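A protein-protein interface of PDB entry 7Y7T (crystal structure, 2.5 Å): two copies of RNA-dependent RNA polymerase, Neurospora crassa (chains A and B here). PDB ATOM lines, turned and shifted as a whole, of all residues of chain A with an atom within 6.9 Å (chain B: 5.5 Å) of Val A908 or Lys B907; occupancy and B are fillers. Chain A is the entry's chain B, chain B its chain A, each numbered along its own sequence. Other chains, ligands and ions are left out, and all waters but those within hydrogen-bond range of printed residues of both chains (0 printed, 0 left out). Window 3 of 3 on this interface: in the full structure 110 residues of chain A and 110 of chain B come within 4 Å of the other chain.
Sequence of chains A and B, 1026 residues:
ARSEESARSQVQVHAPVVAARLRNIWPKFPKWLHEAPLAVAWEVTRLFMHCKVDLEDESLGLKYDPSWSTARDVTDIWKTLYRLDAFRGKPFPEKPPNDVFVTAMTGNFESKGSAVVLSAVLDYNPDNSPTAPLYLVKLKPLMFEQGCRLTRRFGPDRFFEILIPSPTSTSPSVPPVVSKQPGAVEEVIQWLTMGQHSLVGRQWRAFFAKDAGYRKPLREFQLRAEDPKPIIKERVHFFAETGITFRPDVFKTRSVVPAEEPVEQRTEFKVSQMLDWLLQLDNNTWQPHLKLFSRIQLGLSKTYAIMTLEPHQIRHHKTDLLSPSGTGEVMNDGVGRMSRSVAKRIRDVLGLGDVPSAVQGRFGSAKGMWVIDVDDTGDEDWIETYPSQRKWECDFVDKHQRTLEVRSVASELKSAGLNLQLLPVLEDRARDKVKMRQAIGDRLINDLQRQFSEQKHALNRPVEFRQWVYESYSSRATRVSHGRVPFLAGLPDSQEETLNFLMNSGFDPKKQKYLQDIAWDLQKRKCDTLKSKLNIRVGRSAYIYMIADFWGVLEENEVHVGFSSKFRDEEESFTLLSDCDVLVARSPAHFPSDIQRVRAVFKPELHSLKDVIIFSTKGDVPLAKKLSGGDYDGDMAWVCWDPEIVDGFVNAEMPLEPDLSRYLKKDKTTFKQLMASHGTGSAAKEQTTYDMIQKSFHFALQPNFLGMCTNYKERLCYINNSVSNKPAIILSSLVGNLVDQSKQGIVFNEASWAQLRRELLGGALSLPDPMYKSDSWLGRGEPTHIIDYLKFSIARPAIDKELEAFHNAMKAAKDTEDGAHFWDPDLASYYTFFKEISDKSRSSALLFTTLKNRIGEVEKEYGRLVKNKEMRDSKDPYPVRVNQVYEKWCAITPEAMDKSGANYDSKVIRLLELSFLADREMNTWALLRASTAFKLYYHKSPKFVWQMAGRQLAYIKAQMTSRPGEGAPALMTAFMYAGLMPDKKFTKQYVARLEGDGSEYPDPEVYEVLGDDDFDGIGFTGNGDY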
ATOM      1  N   PHE A 833      24.100  24.328  26.416  1.00  0.00           N
ATOM      2  CA  PHE A 833      24.907  23.970  25.253  1.00  0.00           C
ATOM      3  C   PHE A 833      24.277  24.487  23.964  1.00  0.00           C
ATOM      4  O   PHE A 833      24.987  24.917  23.047  1.00  0.00           O
ATOM      5  CB  PHE A 833      25.103  22.450  25.213  1.00  0.00           C
ATOM      6  CG  PHE A 833      25.356  21.888  23.836  1.00  0.00           C
ATOM      7  CD1 PHE A 833      24.306  21.478  23.027  1.00  0.00           C
ATOM      8  CD2 PHE A 833      26.652  21.726  23.369  1.00  0.00           C
ATOM      9  CE1 PHE A 833      24.543  20.956  21.770  1.00  0.00           C
ATOM     10  CE2 PHE A 833      26.893  21.201  22.113  1.00  0.00           C
ATOM     11  CZ  PHE A 833      25.838  20.815  21.313  1.00  0.00           C
ATOM     12  N   PHE A 834      22.943  24.470  23.881  1.00  0.00           N
ATOM     13  CA  PHE A 834      22.275  24.972  22.683  1.00  0.00           C
ATOM     14  C   PHE A 834      22.284  26.495  22.634  1.00  0.00           C
ATOM     15  O   PHE A 834      22.447  27.082  21.557  1.00  0.00           O
ATOM     16  CB  PHE A 834      20.840  24.455  22.612  1.00  0.00           C
ATOM     17  CG  PHE A 834      20.362  24.193  21.213  1.00  0.00           C
ATOM     18  CD1 PHE A 834      20.863  23.131  20.480  1.00  0.00           C
ATOM     19  CD2 PHE A 834      19.430  25.027  20.623  1.00  0.00           C
ATOM     20  CE1 PHE A 834      20.423  22.895  19.190  1.00  0.00           C
ATOM     21  CE2 PHE A 834      18.987  24.798  19.338  1.00  0.00           C
ATOM     22  CZ  PHE A 834      19.483  23.733  18.620  1.00  0.00           C
ATOM     23  N   ILE A 837      25.122  27.571  20.996  1.00  0.00           N
ATOM     24  CA  ILE A 837      24.963  27.398  19.556  1.00  0.00           C
ATOM     25  C   ILE A 837      23.984  28.424  19.001  1.00  0.00           C
ATOM     26  O   ILE A 837      24.232  29.038  17.956  1.00  0.00           O
ATOM     27  CB  ILE A 837      24.515  25.960  19.234  1.00  0.00           C
ATOM     28  CG1 ILE A 837      25.658  24.970  19.483  1.00  0.00           C
ATOM     29  CG2 ILE A 837      24.005  25.868  17.799  1.00  0.00           C
ATOM     30  CD1 ILE A 837      25.559  23.693  18.671  1.00  0.00           C
ATOM     31  N   SER A 841      23.956  31.487  15.947  1.00  0.00           N
ATOM     32  CA  SER A 841      23.223  31.013  14.782  1.00  0.00           C
ATOM     33  C   SER A 841      21.866  31.700  14.688  1.00  0.00           C
ATOM     34  O   SER A 841      21.383  32.310  15.645  1.00  0.00           O
ATOM     35  CB  SER A 841      23.041  29.492  14.823  1.00  0.00           C
ATOM     36  OG  SER A 841      22.158  29.060  13.802  1.00  0.00           O
ATOM     37  N   SER A 843      19.289  29.777  12.659  1.00  0.00           N
ATOM     38  CA  SER A 843      18.374  28.616  12.529  1.00  0.00           C
ATOM     39  C   SER A 843      18.115  28.025  13.906  1.00  0.00           C
ATOM     40  O   SER A 843      16.940  27.809  14.258  1.00  0.00           O
ATOM     41  CB  SER A 843      19.003  27.588  11.637  1.00  0.00           C
ATOM     42  OG  SER A 843      20.392  27.478  11.900  1.00  0.00           O
ATOM     43  N   SER A 844      19.167  27.805  14.668  1.00  0.00           N
ATOM     44  CA  SER A 844      19.039  27.219  16.020  1.00  0.00           C
ATOM     45  C   SER A 844      18.208  28.159  16.886  1.00  0.00           C
ATOM     46  O   SER A 844      17.368  27.664  17.642  1.00  0.00           O
ATOM     47  CB  SER A 844      20.398  26.994  16.603  1.00  0.00           C
ATOM     48  N   LEU A 847      14.469  27.678  16.307  1.00  0.00           N
ATOM     49  CA  LEU A 847      13.992  26.400  16.889  1.00  0.00           C
ATOM     50  C   LEU A 847      13.930  26.559  18.402  1.00  0.00           C
ATOM     51  O   LEU A 847      12.914  26.169  18.992  1.00  0.00           O
ATOM     52  CB  LEU A 847      14.971  25.284  16.518  1.00  0.00           C
ATOM     53  CG  LEU A 847      14.386  23.875  16.470  1.00  0.00           C
ATOM     54  CD1 LEU A 847      13.008  23.883  15.826  1.00  0.00           C
ATOM     55  CD2 LEU A 847      15.319  22.932  15.728  1.00  0.00           C
ATOM     56  N   PRO A 894      10.575  18.566  16.747  1.00  0.00           N
ATOM     57  CA  PRO A 894      11.236  19.387  15.747  1.00  0.00           C
ATOM     58  C   PRO A 894      10.298  19.664  14.565  1.00  0.00           C
ATOM     59  O   PRO A 894      10.368  20.741  14.016  1.00  0.00           O
ATOM     60  CB  PRO A 894      12.397  18.504  15.287  1.00  0.00           C
ATOM     61  CG  PRO A 894      12.724  17.691  16.504  1.00  0.00           C
ATOM     62  CD  PRO A 894      11.361  17.376  17.079  1.00  0.00           C
ATOM     63  N   LYS A 907      19.854  19.551   8.985  1.00  0.00           N
ATOM     64  CA  LYS A 907      20.813  18.502   9.415  1.00  0.00           C
ATOM     65  C   LYS A 907      20.789  18.408  10.941  1.00  0.00           C
ATOM     66  O   LYS A 907      20.844  17.285  11.461  1.00  0.00           O
ATOM     67  CB  LYS A 907      22.217  18.816   8.894  1.00  0.00           C
ATOM     68  N   VAL A 908      20.717  19.545  11.628  1.00  0.00           N
ATOM     69  CA  VAL A 908      20.603  19.530  13.112  1.00  0.00           C
ATOM     70  C   VAL A 908      19.276  18.869  13.485  1.00  0.00           C
ATOM     71  O   VAL A 908      19.270  18.065  14.429  1.00  0.00           O
ATOM     72  CB  VAL A 908      20.730  20.947  13.701  1.00  0.00           C
ATOM     73  CG1 VAL A 908      19.984  21.103  15.016  1.00  0.00           C
ATOM     74  CG2 VAL A 908      22.185  21.352  13.864  1.00  0.00           C
ATOM     75  N   ILE A 909      18.210  19.152  12.735  1.00  0.00           N
ATOM     76  CA  ILE A 909      16.862  18.625  13.100  1.00  0.00           C
ATOM     77  C   ILE A 909      16.926  17.097  13.093  1.00  0.00           C
ATOM     78  O   ILE A 909      16.375  16.474  14.012  1.00  0.00           O
ATOM     79  CB  ILE A 909      15.800  19.165  12.125  1.00  0.00           C
ATOM     80  CG1 ILE A 909      15.438  20.618  12.435  1.00  0.00           C
ATOM     81  CG2 ILE A 909      14.566  18.278  12.102  1.00  0.00           C
ATOM     82  CD1 ILE A 909      13.953  20.890  12.426  1.00  0.00           C
ATOM     83  N   ARG A 910      17.612  16.528  12.107  1.00  0.00           N
ATOM     84  CA  ARG A 910      17.725  15.056  12.009  1.00  0.00           C
ATOM     85  C   ARG A 910      18.477  14.502  13.220  1.00  0.00           C
ATOM     86  O   ARG A 910      18.015  13.495  13.776  1.00  0.00           O
ATOM     87  CB  ARG A 910      18.474  14.688  10.727  1.00  0.00           C
ATOM     88  CG  ARG A 910      17.942  15.374   9.477  1.00  0.00           C
ATOM     89  CD  ARG A 910      17.904  14.443   8.280  1.00  0.00           C
ATOM     90  NE  ARG A 910      19.192  14.347   7.611  1.00  0.00           N
ATOM     91  CZ  ARG A 910      19.463  13.505   6.621  1.00  0.00           C
ATOM     92  NH1 ARG A 910      18.531  12.678   6.181  1.00  0.00           N
ATOM     93  NH2 ARG A 910      20.666  13.492   6.074  1.00  0.00           N
ATOM     94  N   LEU A 911      19.584  15.133  13.611  1.00  0.00           N
ATOM     95  CA  LEU A 911      20.401  14.596  14.726  1.00  0.00           C
ATOM     96  C   LEU A 911      19.568  14.634  16.011  1.00  0.00           C
ATOM     97  O   LEU A 911      19.702  13.723  16.834  1.00  0.00           O
ATOM     98  CB  LEU A 911      21.691  15.407  14.847  1.00  0.00           C
ATOM     99  CG  LEU A 911      22.959  14.709  14.360  1.00  0.00           C
ATOM    100  CD1 LEU A 911      24.136  15.669  14.365  1.00  0.00           C
ATOM    101  CD2 LEU A 911      23.270  13.494  15.217  1.00  0.00           C
ATOM    102  N   LEU A 912      18.789  15.691  16.201  1.00  0.00           N
ATOM    103  CA  LEU A 912      17.914  15.769  17.389  1.00  0.00           C
ATOM    104  C   LEU A 912      16.804  14.719  17.321  1.00  0.00           C
ATOM    105  O   LEU A 912      16.539  14.097  18.355  1.00  0.00           O
ATOM    106  CB  LEU A 912      17.325  17.180  17.435  1.00  0.00           C
ATOM    107  CG  LEU A 912      18.317  18.298  17.747  1.00  0.00           C
ATOM    108  CD1 LEU A 912      17.589  19.612  17.976  1.00  0.00           C
ATOM    109  CD2 LEU A 912      19.165  17.945  18.956  1.00  0.00           C
ATOM    110  N   GLU A 913      16.165  14.552  16.164  1.00  0.00           N
ATOM    111  CA  GLU A 913      15.006  13.623  16.022  1.00  0.00           C
ATOM    112  C   GLU A 913      15.393  12.143  16.140  1.00  0.00           C
ATOM    113  O   GLU A 913      14.594  11.384  16.705  1.00  0.00           O
ATOM    114  CB  GLU A 913      14.220  13.943  14.750  1.00  0.00           C
ATOM    115  CG  GLU A 913      12.730  14.114  14.989  1.00  0.00           C
ATOM    116  CD  GLU A 913      12.011  14.933  13.933  1.00  0.00           C
ATOM    117  OE1 GLU A 913      12.645  15.259  12.912  1.00  0.00           O
ATOM    118  OE2 GLU A 913      10.821  15.245  14.134  1.00  0.00           O
ATOM    119  N   ASP B 905      31.258  21.514   9.525  1.00  0.00           N
ATOM    120  CA  ASP B 905      29.984  22.022  10.029  1.00  0.00           C
ATOM    121  C   ASP B 905      29.990  21.884  11.547  1.00  0.00           C
ATOM    122  O   ASP B 905      29.779  20.796  12.087  1.00  0.00           O
ATOM    123  CB  ASP B 905      28.809  21.281   9.397  1.00  0.00           C
ATOM    124  CG  ASP B 905      29.081  19.803   9.205  1.00  0.00           C
ATOM    125  OD1 ASP B 905      30.245  19.382   9.363  1.00  0.00           O
ATOM    126  OD2 ASP B 905      28.125  19.062   8.891  1.00  0.00           O
ATOM    127  N   SER B 906      30.240  22.998  12.239  1.00  0.00           N
ATOM    128  CA  SER B 906      30.511  22.945  13.673  1.00  0.00           C
ATOM    129  C   SER B 906      29.250  22.654  14.477  1.00  0.00           C
ATOM    130  O   SER B 906      29.314  21.972  15.507  1.00  0.00           O
ATOM    131  CB  SER B 906      31.148  24.257  14.133  1.00  0.00           C
ATOM    132  OG  SER B 906      31.144  24.355  15.546  1.00  0.00           O
ATOM    133  N   LYS B 907      28.103  23.176  14.033  1.00  0.00           N
ATOM    134  CA  LYS B 907      26.828  22.872  14.680  1.00  0.00           C
ATOM    135  C   LYS B 907      26.634  21.372  14.871  1.00  0.00           C
ATOM    136  O   LYS B 907      26.024  20.940  15.856  1.00  0.00           O
ATOM    137  CB  LYS B 907      25.681  23.448  13.847  1.00  0.00           C
ATOM    138  CG  LYS B 907      25.535  22.765  12.493  1.00  0.00           C
ATOM    139  CD  LYS B 907      24.572  23.469  11.566  1.00  0.00           C
ATOM    140  CE  LYS B 907      24.336  22.622  10.325  1.00  0.00           C
ATOM    141  NZ  LYS B 907      25.607  22.367   9.587  1.00  0.00           N
ATOM    142  N   VAL B 908      27.160  20.567  13.946  1.00  0.00           N
ATOM    143  CA  VAL B 908      27.018  19.120  14.021  1.00  0.00           C
ATOM    144  C   VAL B 908      28.110  18.518  14.896  1.00  0.00           C
ATOM    145  O   VAL B 908      27.855  17.596  15.679  1.00  0.00           O
ATOM    146  CB  VAL B 908      27.030  18.529  12.597  1.00  0.00           C
ATOM    147  CG1 VAL B 908      27.310  17.036  12.629  1.00  0.00           C
ATOM    148  CG2 VAL B 908      25.714  18.823  11.889  1.00  0.00           C
ATOM    149  N   ILE B 909      29.323  19.046  14.765  1.00  0.00           N
ATOM    150  CA  ILE B 909      30.471  18.498  15.540  1.00  0.00           C
ATOM    151  C   ILE B 909      30.141  18.645  17.022  1.00  0.00           C
ATOM    152  O   ILE B 909      30.424  17.717  17.782  1.00  0.00           O
ATOM    153  CB  ILE B 909      31.767  19.229  15.153  1.00  0.00           C
ATOM    154  CG1 ILE B 909      32.245  18.815  13.760  1.00  0.00           C
ATOM    155  CG2 ILE B 909      32.853  19.021  16.196  1.00  0.00           C
ATOM    156  CD1 ILE B 909      33.379  17.821  13.780  1.00  0.00           C
ATOM    157  N   ARG B 910      29.556  19.775  17.397  1.00  0.00           N
ATOM    158  CA  ARG B 910      29.222  20.023  18.818  1.00  0.00           C
ATOM    159  C   ARG B 910      28.148  19.041  19.282  1.00  0.00           C
ATOM    160  O   ARG B 910      28.272  18.523  20.404  1.00  0.00           O
ATOM    161  CB  ARG B 910      28.781  21.477  18.995  1.00  0.00           C
ATOM    162  CG  ARG B 910      29.915  22.431  19.342  1.00  0.00           C
ATOM    163  CD  ARG B 910      29.409  23.653  20.082  1.00  0.00           C
ATOM    164  NE  ARG B 910      29.693  23.593  21.509  1.00  0.00           N
ATOM    165  CZ  ARG B 910      28.981  24.213  22.441  1.00  0.00           C
ATOM    166  NH1 ARG B 910      27.933  24.940  22.099  1.00  0.00           N
ATOM    167  NH2 ARG B 910      29.317  24.100  23.714  1.00  0.00           N
ATOM    168  N   LEU B 911      27.138  18.798  18.445  1.00  0.00           N
ATOM    169  CA  LEU B 911      26.036  17.878  18.824  1.00  0.00           C
ATOM    170  C   LEU B 911      26.608  16.474  19.012  1.00  0.00           C
ATOM    171  O   LEU B 911      26.138  15.766  19.904  1.00  0.00           O
ATOM    172  CB  LEU B 911      24.947  17.915  17.753  1.00  0.00           C
ATOM    173  CG  LEU B 911      23.754  18.810  18.073  1.00  0.00           C
ATOM    174  CD1 LEU B 911      22.772  18.834  16.914  1.00  0.00           C
ATOM    175  CD2 LEU B 911      23.065  18.345  19.343  1.00  0.00           C
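NH1 of Arg B910 sits at hydrogen-bond distance from O of Phe A833, at 3.1 Å.
Among the printed residues, merely in contact across the chains: Phe A833 with Leu B911 (3.7 Å), Ile A837 with Lys B907 (3.96 Å), Ile A837 with Arg B910 (3.5 Å), Val A908 with Lys B907 (3.9 Å), Val A908 with Leu B911 (3.998 Å), Leu A911 with Val B908 (3.9 Å) and Leu A912 with Leu B911 (3.9 Å).
Of the printed residues of chain B, Phe A833 touches Arg B910 (3.1 Å) and Leu B911 (3.7 Å).
Printed residues of chain B within 4 Å of Ile A837: Lys B907 (3.96 Å) and Arg B910 (3.5 Å).
Printed residues of chain B within 4 Å of Val A908: Lys B907 (3.9 Å) and Leu B911 (3.998 Å).
Of the printed residues of chain B, Leu A912 touches Leu B911.
Of chain A, only Ile A837 (3.96 Å) and Val A908 (3.9 Å) come within 4 Å of Lys B907.
Printed residues of chain B that touch a printed residue of chain A: Lys B907, Val B908, Arg B910 and Leu B911.
Hydrophobic or aromatic side chains of chain B within 4 Å of the printed part of chain A: Val B908 and Leu B911.
Of the 15 printed residues of chain A, 5 touch a printed residue of chain B.
Printed residues of chain A that touch a printed residue of chain B: Phe A833, Ile A837, Val A908, Leu A911 and Leu A912.
Val A908 touches Lys B907, but with the chains exchanged Lys A907 does not touch Val B908 (4.6 Å).
Val A908 touches Leu B911, and with the chains exchanged Leu A911 touches Val B908.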
